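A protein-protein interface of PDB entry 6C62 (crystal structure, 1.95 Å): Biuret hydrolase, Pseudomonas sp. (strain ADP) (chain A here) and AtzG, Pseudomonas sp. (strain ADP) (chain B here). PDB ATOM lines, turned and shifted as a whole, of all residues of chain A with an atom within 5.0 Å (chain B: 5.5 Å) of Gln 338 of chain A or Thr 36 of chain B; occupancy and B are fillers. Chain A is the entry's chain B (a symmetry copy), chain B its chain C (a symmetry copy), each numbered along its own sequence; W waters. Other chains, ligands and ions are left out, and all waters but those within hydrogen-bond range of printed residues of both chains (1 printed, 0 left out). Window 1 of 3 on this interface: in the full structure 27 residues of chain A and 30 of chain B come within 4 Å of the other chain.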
ATOM      1  N   PHE A 302     -26.284  -2.354 -10.695  1.00  0.00           N
ATOM      2  CA  PHE A 302     -25.481  -3.551 -10.866  1.00  0.00           C
ATOM      3  C   PHE A 302     -24.092  -3.185 -11.397  1.00  0.00           C
ATOM      4  O   PHE A 302     -23.095  -3.655 -10.906  1.00  0.00           O
ATOM      5  CB  PHE A 302     -26.193  -4.523 -11.796  1.00  0.00           C
ATOM      6  CG  PHE A 302     -25.632  -5.893 -11.802  1.00  0.00           C
ATOM      7  CD1 PHE A 302     -24.463  -6.178 -12.486  1.00  0.00           C
ATOM      8  CD2 PHE A 302     -26.284  -6.930 -11.142  1.00  0.00           C
ATOM      9  CE1 PHE A 302     -23.880  -7.431 -12.429  1.00  0.00           C
ATOM     10  CE2 PHE A 302     -25.726  -8.219 -11.132  1.00  0.00           C
ATOM     11  CZ  PHE A 302     -24.522  -8.459 -11.797  1.00  0.00           C
ATOM     12  N   VAL A 303     -24.064  -2.322 -12.411  1.00  0.00           N
ATOM     13  CA  VAL A 303     -22.835  -1.834 -13.002  1.00  0.00           C
ATOM     14  C   VAL A 303     -21.947  -1.079 -12.013  1.00  0.00           C
ATOM     15  O   VAL A 303     -20.753  -1.324 -11.919  1.00  0.00           O
ATOM     16  CB  VAL A 303     -23.153  -1.025 -14.292  1.00  0.00           C
ATOM     17  CG1 VAL A 303     -21.964  -0.229 -14.746  1.00  0.00           C
ATOM     18  CG2 VAL A 303     -23.558  -2.000 -15.410  1.00  0.00           C
ATOM     19  N   ALA A 306     -20.533  -3.469  -9.183  1.00  0.00           N
ATOM     20  CA  ALA A 306     -19.469  -4.378  -9.550  1.00  0.00           C
ATOM     21  C   ALA A 306     -18.144  -3.632  -9.726  1.00  0.00           C
ATOM     22  O   ALA A 306     -17.117  -4.140  -9.291  1.00  0.00           O
ATOM     23  CB  ALA A 306     -19.830  -5.112 -10.821  1.00  0.00           C
ATOM     24  N   SER A 307     -18.146  -2.487 -10.377  1.00  0.00           N
ATOM     25  CA  SER A 307     -16.881  -1.755 -10.531  1.00  0.00           C
ATOM     26  C   SER A 307     -16.336  -1.174  -9.227  1.00  0.00           C
ATOM     27  O   SER A 307     -15.138  -1.285  -8.963  1.00  0.00           O
ATOM     28  CB  SER A 307     -17.040  -0.668 -11.592  1.00  0.00           C
ATOM     29  OG  SER A 307     -17.059  -1.305 -12.898  1.00  0.00           O
ATOM     30  N   SER A 334     -14.775  -9.596 -12.717  1.00  0.00           N
ATOM     31  CA  SER A 334     -15.589  -9.046 -13.785  1.00  0.00           C
ATOM     32  C   SER A 334     -15.853  -7.564 -13.621  1.00  0.00           C
ATOM     33  O   SER A 334     -15.688  -6.785 -14.562  1.00  0.00           O
ATOM     34  CB  SER A 334     -16.929  -9.815 -13.860  1.00  0.00           C
ATOM     35  OG  SER A 334     -17.753  -9.282 -14.886  1.00  0.00           O
ATOM     36  N   GLY A 335     -16.210  -7.172 -12.404  1.00  0.00           N
ATOM     37  CA  GLY A 335     -16.446  -5.748 -12.094  1.00  0.00           C
ATOM     38  C   GLY A 335     -15.247  -4.855 -12.374  1.00  0.00           C
ATOM     39  O   GLY A 335     -15.389  -3.740 -12.947  1.00  0.00           O
ATOM     40  N   VAL A 336     -14.050  -5.327 -11.991  1.00  0.00           N
ATOM     41  CA  VAL A 336     -12.803  -4.554 -12.255  1.00  0.00           C
ATOM     42  C   VAL A 336     -12.581  -4.353 -13.777  1.00  0.00           C
ATOM     43  O   VAL A 336     -12.006  -3.324 -14.191  1.00  0.00           O
ATOM     44  CB  VAL A 336     -11.604  -5.287 -11.695  1.00  0.00           C
ATOM     45  CG1 VAL A 336     -10.320  -4.641 -12.121  1.00  0.00           C
ATOM     46  CG2 VAL A 336     -11.633  -5.276 -10.203  1.00  0.00           C
ATOM     47  N   LEU A 337     -12.988  -5.358 -14.581  1.00  0.00           N
ATOM     48  CA  LEU A 337     -12.764  -5.327 -16.022  1.00  0.00           C
ATOM     49  C   LEU A 337     -13.820  -4.576 -16.838  1.00  0.00           C
ATOM     50  O   LEU A 337     -13.684  -4.441 -18.053  1.00  0.00           O
ATOM     51  CB  LEU A 337     -12.534  -6.744 -16.570  1.00  0.00           C
ATOM     52  CG  LEU A 337     -11.497  -7.585 -15.811  1.00  0.00           C
ATOM     53  CD1 LEU A 337     -11.218  -8.980 -16.426  1.00  0.00           C
ATOM     54  CD2 LEU A 337     -10.200  -6.847 -15.786  1.00  0.00           C
ATOM     55  N   GLN A 338     -14.844  -4.025 -16.182  1.00  0.00           N
ATOM     56  CA  GLN A 338     -15.918  -3.338 -16.878  1.00  0.00           C
ATOM     57  C   GLN A 338     -15.423  -2.059 -17.496  1.00  0.00           C
ATOM     58  O   GLN A 338     -14.701  -1.298 -16.857  1.00  0.00           O
ATOM     59  CB  GLN A 338     -17.104  -3.060 -15.964  1.00  0.00           C
ATOM     60  CG  GLN A 338     -17.905  -4.259 -15.548  1.00  0.00           C
ATOM     61  CD  GLN A 338     -18.935  -3.934 -14.491  1.00  0.00           C
ATOM     62  OE1 GLN A 338     -19.512  -4.864 -13.946  1.00  0.00           O
ATOM     63  NE2 GLN A 338     -19.202  -2.639 -14.217  1.00  0.00           N
ATOM     64  N   PRO A 339     -15.748  -1.836 -18.787  1.00  0.00           N
ATOM     65  CA  PRO A 339     -15.389  -0.551 -19.393  1.00  0.00           C
ATOM     66  C   PRO A 339     -15.845   0.670 -18.488  1.00  0.00           C
ATOM     67  O   PRO A 339     -16.940   0.673 -17.887  1.00  0.00           O
ATOM     68  CB  PRO A 339     -16.210  -0.572 -20.726  1.00  0.00           C
ATOM     69  CG  PRO A 339     -16.302  -2.012 -21.086  1.00  0.00           C
ATOM     70  CD  PRO A 339     -16.362  -2.771 -19.756  1.00  0.00           C
ATOM     71  N   VAL A 340     -15.000   1.680 -18.440  1.00  0.00           N
ATOM     72  CA  VAL A 340     -15.315   2.929 -17.779  1.00  0.00           C
ATOM     73  C   VAL A 340     -16.573   3.552 -18.387  1.00  0.00           C
ATOM     74  O   VAL A 340     -17.329   4.218 -17.683  1.00  0.00           O
ATOM     75  CB  VAL A 340     -14.130   3.864 -17.780  1.00  0.00           C
ATOM     76  CG1 VAL A 340     -13.859   4.426 -19.182  1.00  0.00           C
ATOM     77  CG2 VAL A 340     -14.343   5.018 -16.794  1.00  0.00           C
ATOM     78  N   TRP A 342     -19.354   2.225 -19.106  1.00  0.00           N
ATOM     79  CA  TRP A 342     -20.570   1.654 -18.457  1.00  0.00           C
ATOM     80  C   TRP A 342     -20.780   2.355 -17.130  1.00  0.00           C
ATOM     81  O   TRP A 342     -21.928   2.773 -16.815  1.00  0.00           O
ATOM     82  CB  TRP A 342     -20.439   0.179 -18.193  1.00  0.00           C
ATOM     83  CG  TRP A 342     -20.243  -0.678 -19.414  1.00  0.00           C
ATOM     84  CD1 TRP A 342     -20.314  -0.296 -20.687  1.00  0.00           C
ATOM     85  CD2 TRP A 342     -20.065  -2.093 -19.427  1.00  0.00           C
ATOM     86  NE1 TRP A 342     -20.139  -1.389 -21.521  1.00  0.00           N
ATOM     87  CE2 TRP A 342     -19.972  -2.493 -20.752  1.00  0.00           C
ATOM     88  CE3 TRP A 342     -20.035  -3.074 -18.417  1.00  0.00           C
ATOM     89  CZ2 TRP A 342     -19.823  -3.839 -21.133  1.00  0.00           C
ATOM     90  CZ3 TRP A 342     -19.865  -4.413 -18.776  1.00  0.00           C
ATOM     91  CH2 TRP A 342     -19.758  -4.788 -20.113  1.00  0.00           C
ATOM     92  N   TYR B   9     -11.014  -9.908 -24.708  1.00  0.00           N
ATOM     93  CA  TYR B   9     -11.012  -8.723 -23.840  1.00  0.00           C
ATOM     94  C   TYR B   9     -10.672  -9.067 -22.369  1.00  0.00           C
ATOM     95  O   TYR B   9      -9.845  -8.402 -21.756  1.00  0.00           O
ATOM     96  CB  TYR B   9     -12.359  -8.003 -23.918  1.00  0.00           C
ATOM     97  CG  TYR B   9     -12.421  -6.837 -22.969  1.00  0.00           C
ATOM     98  CD1 TYR B   9     -11.712  -5.684 -23.229  1.00  0.00           C
ATOM     99  CD2 TYR B   9     -13.116  -6.916 -21.755  1.00  0.00           C
ATOM    100  CE1 TYR B   9     -11.736  -4.611 -22.363  1.00  0.00           C
ATOM    101  CE2 TYR B   9     -13.159  -5.860 -20.893  1.00  0.00           C
ATOM    102  CZ  TYR B   9     -12.458  -4.702 -21.204  1.00  0.00           C
ATOM    103  OH  TYR B   9     -12.469  -3.612 -20.333  1.00  0.00           O
ATOM    104  N   HIS B  32     -19.712 -14.201 -16.144  1.00  0.00           N
ATOM    105  CA  HIS B  32     -20.352 -13.107 -15.430  1.00  0.00           C
ATOM    106  C   HIS B  32     -20.343 -11.847 -16.289  1.00  0.00           C
ATOM    107  O   HIS B  32     -21.342 -11.101 -16.318  1.00  0.00           O
ATOM    108  CB  HIS B  32     -19.678 -12.833 -14.074  1.00  0.00           C
ATOM    109  CG  HIS B  32     -19.754 -13.997 -13.130  1.00  0.00           C
ATOM    110  ND1 HIS B  32     -20.940 -14.415 -12.592  1.00  0.00           N
ATOM    111  CD2 HIS B  32     -18.801 -14.819 -12.624  1.00  0.00           C
ATOM    112  CE1 HIS B  32     -20.731 -15.466 -11.807  1.00  0.00           C
ATOM    113  NE2 HIS B  32     -19.435 -15.739 -11.816  1.00  0.00           N
ATOM    114  N   PHE B  33     -19.204 -11.556 -16.922  1.00  0.00           N
ATOM    115  CA  PHE B  33     -19.064 -10.371 -17.709  1.00  0.00           C
ATOM    116  C   PHE B  33     -20.096 -10.283 -18.824  1.00  0.00           C
ATOM    117  O   PHE B  33     -20.623  -9.205 -19.093  1.00  0.00           O
ATOM    118  CB  PHE B  33     -17.699 -10.309 -18.306  1.00  0.00           C
ATOM    119  CG  PHE B  33     -17.407  -9.054 -19.021  1.00  0.00           C
ATOM    120  CD1 PHE B  33     -17.681  -8.931 -20.375  1.00  0.00           C
ATOM    121  CD2 PHE B  33     -16.795  -7.993 -18.367  1.00  0.00           C
ATOM    122  CE1 PHE B  33     -17.395  -7.761 -21.025  1.00  0.00           C
ATOM    123  CE2 PHE B  33     -16.427  -6.858 -19.067  1.00  0.00           C
ATOM    124  CZ  PHE B  33     -16.722  -6.731 -20.371  1.00  0.00           C
ATOM    125  N   SER B  34     -20.400 -11.416 -19.446  1.00  0.00           N
ATOM    126  CA  SER B  34     -21.404 -11.456 -20.509  1.00  0.00           C
ATOM    127  C   SER B  34     -22.791 -11.041 -20.066  1.00  0.00           C
ATOM    128  O   SER B  34     -23.525 -10.368 -20.820  1.00  0.00           O
ATOM    129  CB  SER B  34     -21.461 -12.865 -21.120  1.00  0.00           C
ATOM    130  OG  SER B  34     -20.273 -13.096 -21.837  1.00  0.00           O
ATOM    131  N   ARG B  35     -23.168 -11.482 -18.869  1.00  0.00           N
ATOM    132  CA  ARG B  35     -24.470 -11.053 -18.286  1.00  0.00           C
ATOM    133  C   ARG B  35     -24.492  -9.546 -18.022  1.00  0.00           C
ATOM    134  O   ARG B  35     -25.469  -8.856 -18.329  1.00  0.00           O
ATOM    135  CB  ARG B  35     -24.811 -11.803 -16.983  1.00  0.00           C
ATOM    136  CG  ARG B  35     -24.863 -13.337 -17.203  1.00  0.00           C
ATOM    137  CD  ARG B  35     -25.215 -14.137 -15.958  1.00  0.00           C
ATOM    138  NE  ARG B  35     -26.554 -13.713 -15.572  1.00  0.00           N
ATOM    139  CZ  ARG B  35     -27.721 -14.202 -16.054  1.00  0.00           C
ATOM    140  NH1 ARG B  35     -27.748 -15.225 -16.939  1.00  0.00           N
ATOM    141  NH2 ARG B  35     -28.861 -13.643 -15.654  1.00  0.00           N
ATOM    142  N   THR B  36     -23.406  -9.044 -17.463  1.00  0.00           N
ATOM    143  CA  THR B  36     -23.257  -7.586 -17.238  1.00  0.00           C
ATOM    144  C   THR B  36     -23.273  -6.775 -18.544  1.00  0.00           C
ATOM    145  O   THR B  36     -23.853  -5.717 -18.599  1.00  0.00           O
ATOM    146  CB  THR B  36     -22.019  -7.267 -16.418  1.00  0.00           C
ATOM    147  OG1 THR B  36     -22.036  -8.080 -15.251  1.00  0.00           O
ATOM    148  CG2 THR B  36     -22.004  -5.768 -16.028  1.00  0.00           C
ATOM    149  N   ALA B  37     -22.639  -7.292 -19.594  1.00  0.00           N
ATOM    150  CA  ALA B  37     -22.654  -6.610 -20.899  1.00  0.00           C
ATOM    151  C   ALA B  37     -24.086  -6.399 -21.422  1.00  0.00           C
ATOM    152  O   ALA B  37     -24.329  -5.392 -22.052  1.00  0.00           O
ATOM    153  CB  ALA B  37     -21.804  -7.387 -21.917  1.00  0.00           C
ATOM    154  N   LEU B  38     -25.009  -7.332 -21.182  1.00  0.00           N
ATOM    155  CA  LEU B  38     -26.406  -7.168 -21.583  1.00  0.00           C
ATOM    156  C   LEU B  38     -27.066  -6.063 -20.784  1.00  0.00           C
ATOM    157  O   LEU B  38     -27.820  -5.252 -21.329  1.00  0.00           O
ATOM    158  CB  LEU B  38     -27.205  -8.444 -21.397  1.00  0.00           C
ATOM    159  CG  LEU B  38     -26.852  -9.554 -22.381  1.00  0.00           C
ATOM    160  CD1 LEU B  38     -27.495 -10.877 -21.910  1.00  0.00           C
ATOM    161  CD2 LEU B  38     -27.291  -9.145 -23.822  1.00  0.00           C
ATOM    162  N   LEU B  39     -26.752  -5.979 -19.487  1.00  0.00           N
ATOM    163  CA  LEU B  39     -27.225  -4.858 -18.671  1.00  0.00           C
ATOM    164  C   LEU B  39     -26.718  -3.526 -19.172  1.00  0.00           C
ATOM    165  O   LEU B  39     -27.486  -2.543 -19.255  1.00  0.00           O
ATOM    166  CB  LEU B  39     -26.887  -5.064 -17.178  1.00  0.00           C
ATOM    167  CG  LEU B  39     -27.433  -6.301 -16.532  1.00  0.00           C
ATOM    168  CD1 LEU B  39     -27.032  -6.352 -15.061  1.00  0.00           C
ATOM    169  CD2 LEU B  39     -28.926  -6.333 -16.566  1.00  0.00           C
ATOM    170  N   ALA B  40     -25.448  -3.465 -19.524  1.00  0.00           N
ATOM    171  CA  ALA B  40     -24.853  -2.203 -19.965  1.00  0.00           C
ATOM    172  C   ALA B  40     -25.466  -1.765 -21.289  1.00  0.00           C
ATOM    173  O   ALA B  40     -25.667  -0.585 -21.511  1.00  0.00           O
ATOM    174  CB  ALA B  40     -23.332  -2.367 -20.139  1.00  0.00           C
ATOM    175  N   GLU B  41     -25.758  -2.727 -22.144  1.00  0.00           N
ATOM    176  CA  GLU B  41     -26.390  -2.498 -23.406  1.00  0.00           C
ATOM    177  C   GLU B  41     -27.766  -1.897 -23.247  1.00  0.00           C
ATOM    178  O   GLU B  41     -28.116  -0.972 -23.920  1.00  0.00           O
ATOM    179  CB  GLU B  41     -26.442  -3.771 -24.216  1.00  0.00           C
ATOM    180  CG  GLU B  41     -27.060  -3.527 -25.603  1.00  0.00           C
ATOM    181  CD  GLU B  41     -26.220  -3.964 -26.824  1.00  0.00           C
ATOM    182  OE1 GLU B  41     -25.527  -5.027 -26.792  1.00  0.00           O
ATOM    183  OE2 GLU B  41     -26.306  -3.214 -27.837  1.00  0.00           O
HETATM  184  O   HOH W   1     -19.535  -7.647 -13.882  1.00  0.00           O
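OG of Ser 334 of chain A sits close to N of Phe 33 of chain B, 3.4 Å away.
O of Leu 337 of chain A is in hydrogen-bond range of OH of Tyr 9 of chain B.
The backbone carbonyl oxygen (O) of Val 303 of chain A is in hydrogen-bond range of the side-chain amide nitrogen (NE2) of Gln 338 of chain A (3.1 Å).
The side-chain hydroxyl (OG1) of Thr 36 of chain B sits at hydrogen-bond distance from the backbone carbonyl oxygen (O) of His 32 of chain B (3.3 Å).
The side-chain hydroxyl of Ser 307 of chain A is in hydrogen-bond range of the side-chain amide nitrogen of Gln 338 of chain A, 2.8 Å away.
Among the printed residues, merely in contact across the chains: Phe 302 of chain A with Thr 36 of chain B (3.4 Å), Phe 302 of chain A with Leu 39 of chain B (3.6 Å), Ser 334 of chain A with His 32 of chain B (3.9 Å), Leu 337 of chain A with Phe 33 of chain B (3.8 Å), Gln 338 of chain A with Thr 36 of chain B (3.4 Å), Trp 342 of chain A with Phe 33 of chain B (3.6 Å), Trp 342 of chain A with Thr 36 of chain B (3.7 Å), Trp 342 of chain A with Ala 37 of chain B (3.5 Å) and Trp 342 of chain A with Ala 40 of chain B (3.4 Å).
Gln 338 of chain A touches just one residue of chain B: Thr 36.
Of chain A, only Phe 302, Gln 338 and Trp 342 come within 4 Å of Thr 36 of chain B.
Printed residues of chain B within 4 Å of Phe 302 of chain A: Thr 36 (3.4 Å) and Leu 39 (3.6 Å).
Of the printed residues of chain A, Ala 37 of chain B touches Trp 342.
Printed residues of chain B within 4 Å of Leu 337 of chain A: Tyr 9 (2.7 Å) and Phe 33 (3.8 Å).
Glu 41 of chain B touches none of the printed residues of chain A.
Ser 34 of chain B touches none of the printed residues of chain A.
The nearest residue of chain B that does not touch Gln 338 of chain A is Phe 33 of chain B (4.2 Å).
The nearest printed residue of chain A that does not touch His 32 of chain B is Phe 302 of chain A (5.9 Å).
Of the 12 printed residues of chain A, 5 touch a printed residue of chain B.
Hydrophobic or aromatic side chains of chain A within 4 Å of the printed part of chain B: Phe 302 and Trp 342.
Hydrophobic or aromatic side chains of chain B that line the printed part of chain A: Tyr 9, Phe 33, Ala 37, Leu 39 and Ala 40.
Among the printed residues, no Asp or Glu carboxylate lies within 4 Å of a Lys or Arg side-chain nitrogen of the other chain.
Water W1 lies within hydrogen-bond range of the side-chain hydroxyl (OG) of Ser 334 of chain A, the side-chain amide oxygen (OE1) of Gln 338 of chain A and the side-chain hydroxyl (OG1) of Thr 36 of chain B.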
